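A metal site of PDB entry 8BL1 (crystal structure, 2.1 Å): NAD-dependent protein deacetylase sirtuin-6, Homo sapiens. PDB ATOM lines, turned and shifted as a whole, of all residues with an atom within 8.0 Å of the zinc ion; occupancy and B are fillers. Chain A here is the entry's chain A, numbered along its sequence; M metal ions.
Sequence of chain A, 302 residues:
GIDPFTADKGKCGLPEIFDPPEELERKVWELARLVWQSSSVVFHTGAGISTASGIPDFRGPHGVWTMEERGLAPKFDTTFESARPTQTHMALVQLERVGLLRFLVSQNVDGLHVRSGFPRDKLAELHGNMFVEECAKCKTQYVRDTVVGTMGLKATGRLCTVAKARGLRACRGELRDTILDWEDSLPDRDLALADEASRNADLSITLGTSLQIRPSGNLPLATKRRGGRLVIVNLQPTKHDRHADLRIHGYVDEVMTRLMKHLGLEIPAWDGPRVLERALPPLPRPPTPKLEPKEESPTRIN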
ATOM      1  N   GLU A 134      18.961   7.901   8.457  1.00  0.00           N
ATOM      2  CA  GLU A 134      17.516   8.082   8.771  1.00  0.00           C
ATOM      3  C   GLU A 134      16.720   7.944   7.469  1.00  0.00           C
ATOM      4  O   GLU A 134      17.162   8.501   6.430  1.00  0.00           O
ATOM      5  CB  GLU A 134      17.325   9.447   9.461  1.00  0.00           C
ATOM      6  CG  GLU A 134      15.881   9.808   9.718  1.00  0.00           C
ATOM      7  CD  GLU A 134      15.614  11.001  10.636  1.00  0.00           C
ATOM      8  OE1 GLU A 134      16.366  11.185  11.610  1.00  0.00           O
ATOM      9  OE2 GLU A 134      14.624  11.719  10.379  1.00  0.00           O
ATOM     10  N   CYS A 135      15.590   7.233   7.493  1.00  0.00           N
ATOM     11  CA  CYS A 135      14.660   7.088   6.332  1.00  0.00           C
ATOM     12  C   CYS A 135      13.888   8.392   6.167  1.00  0.00           C
ATOM     13  O   CYS A 135      13.309   8.863   7.150  1.00  0.00           O
ATOM     14  CB  CYS A 135      13.704   5.905   6.517  1.00  0.00           C
ATOM     15  SG  CYS A 135      12.388   5.760   5.279  1.00  0.00           S
ATOM     16  N   ALA A 136      13.893   8.957   4.963  1.00  0.00           N
ATOM     17  CA  ALA A 136      13.193  10.221   4.625  1.00  0.00           C
ATOM     18  C   ALA A 136      11.673  10.064   4.792  1.00  0.00           C
ATOM     19  O   ALA A 136      11.015  11.089   5.044  1.00  0.00           O
ATOM     20  CB  ALA A 136      13.547  10.638   3.218  1.00  0.00           C
ATOM     21  N   LYS A 137      11.142   8.850   4.686  1.00  0.00           N
ATOM     22  CA  LYS A 137       9.680   8.576   4.769  1.00  0.00           C
ATOM     23  C   LYS A 137       9.277   8.308   6.222  1.00  0.00           C
ATOM     24  O   LYS A 137       8.600   9.172   6.801  1.00  0.00           O
ATOM     25  CB  LYS A 137       9.290   7.383   3.884  1.00  0.00           C
ATOM     26  CG  LYS A 137       9.547   7.586   2.399  1.00  0.00           C
ATOM     27  CD  LYS A 137       8.907   6.511   1.550  1.00  0.00           C
ATOM     28  CE  LYS A 137       8.922   6.841   0.071  1.00  0.00           C
ATOM     29  NZ  LYS A 137       8.373   5.734  -0.744  1.00  0.00           N
ATOM     30  N   CYS A 138       9.678   7.167   6.790  1.00  0.00           N
ATOM     31  CA  CYS A 138       9.207   6.709   8.119  1.00  0.00           C
ATOM     32  C   CYS A 138      10.092   7.283   9.239  1.00  0.00           C
ATOM     33  O   CYS A 138       9.744   7.047  10.407  1.00  0.00           O
ATOM     34  CB  CYS A 138       9.102   5.195   8.192  1.00  0.00           C
ATOM     35  SG  CYS A 138      10.683   4.302   8.089  1.00  0.00           S
ATOM     36  N   LYS A 139      11.169   7.998   8.903  1.00  0.00           N
ATOM     37  CA  LYS A 139      12.051   8.694   9.883  1.00  0.00           C
ATOM     38  C   LYS A 139      12.743   7.662  10.779  1.00  0.00           C
ATOM     39  O   LYS A 139      13.275   8.068  11.824  1.00  0.00           O
ATOM     40  CB  LYS A 139      11.240   9.706  10.708  1.00  0.00           C
ATOM     41  CG  LYS A 139      10.429  10.696   9.895  1.00  0.00           C
ATOM     42  CD  LYS A 139      11.253  11.538   8.938  1.00  0.00           C
ATOM     43  CE  LYS A 139      10.420  12.505   8.131  1.00  0.00           C
ATOM     44  NZ  LYS A 139      11.200  13.136   7.043  1.00  0.00           N
ATOM     45  N   THR A 140      12.753   6.376  10.367  1.00  0.00           N
ATOM     46  CA  THR A 140      13.413   5.273  11.105  1.00  0.00           C
ATOM     47  C   THR A 140      14.917   5.433  10.986  1.00  0.00           C
ATOM     48  O   THR A 140      15.383   5.723   9.866  1.00  0.00           O
ATOM     49  CB  THR A 140      13.006   3.883  10.579  1.00  0.00           C
ATOM     50  OG1 THR A 140      11.629   3.719  10.879  1.00  0.00           O
ATOM     51  CG2 THR A 140      13.805   2.760  11.207  1.00  0.00           C
ATOM     52  N   GLN A 141      15.620   5.255  12.098  1.00  0.00           N
ATOM     53  CA  GLN A 141      17.081   5.469  12.217  1.00  0.00           C
ATOM     54  C   GLN A 141      17.767   4.104  12.247  1.00  0.00           C
ATOM     55  O   GLN A 141      17.177   3.150  12.763  1.00  0.00           O
ATOM     56  CB  GLN A 141      17.418   6.272  13.482  1.00  0.00           C
ATOM     57  CG  GLN A 141      16.739   7.628  13.533  1.00  0.00           C
ATOM     58  CD  GLN A 141      17.399   8.622  14.454  1.00  0.00           C
ATOM     59  OE1 GLN A 141      17.649   8.342  15.629  1.00  0.00           O
ATOM     60  NE2 GLN A 141      17.604   9.831  13.956  1.00  0.00           N
ATOM     61  N   TYR A 142      18.963   4.029  11.685  1.00  0.00           N
ATOM     62  CA  TYR A 142      19.809   2.815  11.691  1.00  0.00           C
ATOM     63  C   TYR A 142      21.185   3.174  12.254  1.00  0.00           C
ATOM     64  O   TYR A 142      21.786   4.172  11.802  1.00  0.00           O
ATOM     65  CB  TYR A 142      19.940   2.291  10.267  1.00  0.00           C
ATOM     66  CG  TYR A 142      18.634   1.931   9.603  1.00  0.00           C
ATOM     67  CD1 TYR A 142      17.837   2.906   9.035  1.00  0.00           C
ATOM     68  CD2 TYR A 142      18.203   0.613   9.551  1.00  0.00           C
ATOM     69  CE1 TYR A 142      16.627   2.577   8.416  1.00  0.00           C
ATOM     70  CE2 TYR A 142      16.998   0.271   8.932  1.00  0.00           C
ATOM     71  CZ  TYR A 142      16.218   1.261   8.367  1.00  0.00           C
ATOM     72  OH  TYR A 142      15.048   0.925   7.754  1.00  0.00           O
ATOM     73  N   LEU A 159      18.366   1.835   1.020  1.00  0.00           N
ATOM     74  CA  LEU A 159      16.888   1.981   1.147  1.00  0.00           C
ATOM     75  C   LEU A 159      16.444   1.336   2.467  1.00  0.00           C
ATOM     76  O   LEU A 159      17.180   0.480   2.987  1.00  0.00           O
ATOM     77  CB  LEU A 159      16.197   1.282  -0.027  1.00  0.00           C
ATOM     78  CG  LEU A 159      16.662   1.682  -1.418  1.00  0.00           C
ATOM     79  CD1 LEU A 159      15.989   0.836  -2.481  1.00  0.00           C
ATOM     80  CD2 LEU A 159      16.389   3.158  -1.669  1.00  0.00           C
ATOM     81  N   CYS A 160      15.262   1.730   2.935  1.00  0.00           N
ATOM     82  CA  CYS A 160      14.634   1.355   4.231  1.00  0.00           C
ATOM     83  C   CYS A 160      14.120  -0.092   4.195  1.00  0.00           C
ATOM     84  O   CYS A 160      13.558  -0.486   3.165  1.00  0.00           O
ATOM     85  CB  CYS A 160      13.490   2.316   4.511  1.00  0.00           C
ATOM     86  SG  CYS A 160      12.917   2.244   6.225  1.00  0.00           S
ATOM     87  N   THR A 161      14.286  -0.855   5.290  1.00  0.00           N
ATOM     88  CA  THR A 161      13.895  -2.279   5.403  1.00  0.00           C
ATOM     89  C   THR A 161      12.656  -2.442   6.299  1.00  0.00           C
ATOM     90  O   THR A 161      12.284  -3.590   6.530  1.00  0.00           O
ATOM     91  CB  THR A 161      15.070  -3.142   5.917  1.00  0.00           C
ATOM     92  OG1 THR A 161      15.463  -2.718   7.225  1.00  0.00           O
ATOM     93  CG2 THR A 161      16.268  -3.080   4.994  1.00  0.00           C
ATOM     94  N   VAL A 162      12.046  -1.360   6.781  1.00  0.00           N
ATOM     95  CA  VAL A 162      10.894  -1.412   7.732  1.00  0.00           C
ATOM     96  C   VAL A 162       9.781  -2.264   7.100  1.00  0.00           C
ATOM     97  O   VAL A 162       9.450  -2.015   5.932  1.00  0.00           O
ATOM     98  CB  VAL A 162      10.393   0.004   8.113  1.00  0.00           C
ATOM     99  CG1 VAL A 162       8.976  -0.022   8.672  1.00  0.00           C
ATOM    100  CG2 VAL A 162      11.329   0.675   9.101  1.00  0.00           C
ATOM    101  N   ALA A 163       9.234  -3.213   7.874  1.00  0.00           N
ATOM    102  CA  ALA A 163       8.228  -4.214   7.427  1.00  0.00           C
ATOM    103  C   ALA A 163       7.036  -3.508   6.766  1.00  0.00           C
ATOM    104  O   ALA A 163       6.409  -2.673   7.444  1.00  0.00           O
ATOM    105  CB  ALA A 163       7.781  -5.064   8.592  1.00  0.00           C
ATOM    106  N   CYS A 171       9.146  -0.475   3.130  1.00  0.00           N
ATOM    107  CA  CYS A 171       9.101   1.001   2.983  1.00  0.00           C
ATOM    108  C   CYS A 171       9.946   1.417   1.770  1.00  0.00           C
ATOM    109  O   CYS A 171       9.453   2.234   0.971  1.00  0.00           O
ATOM    110  CB  CYS A 171       9.553   1.675   4.273  1.00  0.00           C
ATOM    111  SG  CYS A 171       9.887   3.446   4.106  1.00  0.00           S
ATOM    112  N   ARG A 172      11.173   0.889   1.650  1.00  0.00           N
ATOM    113  CA  ARG A 172      12.149   1.193   0.566  1.00  0.00           C
ATOM    114  C   ARG A 172      12.418   2.710   0.517  1.00  0.00           C
ATOM    115  O   ARG A 172      12.992   3.183  -0.473  1.00  0.00           O
ATOM    116  CB  ARG A 172      11.663   0.626  -0.778  1.00  0.00           C
ATOM    117  CG  ARG A 172      11.159  -0.813  -0.692  1.00  0.00           C
ATOM    118  CD  ARG A 172      11.415  -1.682  -1.911  1.00  0.00           C
ATOM    119  NE  ARG A 172      11.581  -0.912  -3.139  1.00  0.00           N
ATOM    120  CZ  ARG A 172      12.688  -0.846  -3.874  1.00  0.00           C
ATOM    121  NH1 ARG A 172      13.766  -1.542  -3.553  1.00  0.00           N
ATOM    122  NH2 ARG A 172      12.700  -0.076  -4.952  1.00  0.00           N
ATOM    123  N   GLY A 173      12.094   3.434   1.592  1.00  0.00           N
ATOM    124  CA  GLY A 173      12.420   4.859   1.712  1.00  0.00           C
ATOM    125  C   GLY A 173      13.913   5.081   1.552  1.00  0.00           C
ATOM    126  O   GLY A 173      14.699   4.210   1.978  1.00  0.00           O
ATOM    127  N   GLU A 174      14.287   6.214   0.946  1.00  0.00           N
ATOM    128  CA  GLU A 174      15.689   6.634   0.735  1.00  0.00           C
ATOM    129  C   GLU A 174      16.309   6.965   2.096  1.00  0.00           C
ATOM    130  O   GLU A 174      15.736   7.815   2.832  1.00  0.00           O
ATOM    131  CB  GLU A 174      15.719   7.794  -0.244  1.00  0.00           C
ATOM    132  CG  GLU A 174      17.101   8.180  -0.741  1.00  0.00           C
ATOM    133  CD  GLU A 174      17.042   9.264  -1.796  1.00  0.00           C
ATOM    134  OE1 GLU A 174      16.660   8.942  -2.939  1.00  0.00           O
ATOM    135  OE2 GLU A 174      17.376  10.428  -1.476  1.00  0.00           O
ATOM    136  N   LEU A 175      17.423   6.307   2.443  1.00  0.00           N
ATOM    137  CA  LEU A 175      18.210   6.575   3.675  1.00  0.00           C
ATOM    138  C   LEU A 175      19.122   7.783   3.414  1.00  0.00           C
ATOM    139  O   LEU A 175      19.664   7.898   2.292  1.00  0.00           O
ATOM    140  CB  LEU A 175      19.010   5.328   4.058  1.00  0.00           C
ATOM    141  CG  LEU A 175      18.189   4.074   4.393  1.00  0.00           C
ATOM    142  CD1 LEU A 175      19.096   2.940   4.844  1.00  0.00           C
ATOM    143  CD2 LEU A 175      17.156   4.331   5.478  1.00  0.00           C
HETATM  144 ZN    ZN M   1      11.314   3.806   6.031  1.00  0.00          ZN
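Of the 19 residues printed, 4 come within 4 Å of the zinc ion.
Along chain A the residues within 4 Å of the zinc ion span positions 135 to 171.
The zinc ion is bound by SG of Cys 138, at 2.2 Å.
The zinc ion is bound by SG of Cys 160, 2.2 Å away.
The zinc ion is bound by the side-chain sulfur (SG) of Cys 135 (2.4 Å).
The side-chain sulfur (SG) of Cys 171 binds the zinc ion, at 2.4 Å.
The side-chain sulfur (SG) of Cys 138 sits close to the side-chain hydroxyl (OG1) of Thr 140 (3.0 Å).
The backbone NH of Val 162 sits close to the side-chain sulfur of Cys 160, 3.7 Å away.
N of Cys 160 is in hydrogen-bond range of O of Gly 173 (2.7 Å).
SG of Cys 160 sits close to OH of Tyr 142.
N of Arg 172 lies within hydrogen-bond range of O of Cys 160.
The side-chain sulfur (SG) of Cys 135 sits close to the backbone NH (N) of Lys 137, 3.4 Å away.
N of Cys 135 sits at hydrogen-bond distance from O of Thr 140.
The backbone carbonyl oxygen (O) of Val 162 lies within hydrogen-bond range of the backbone NH (N) of Cys 171 (3.2 Å).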
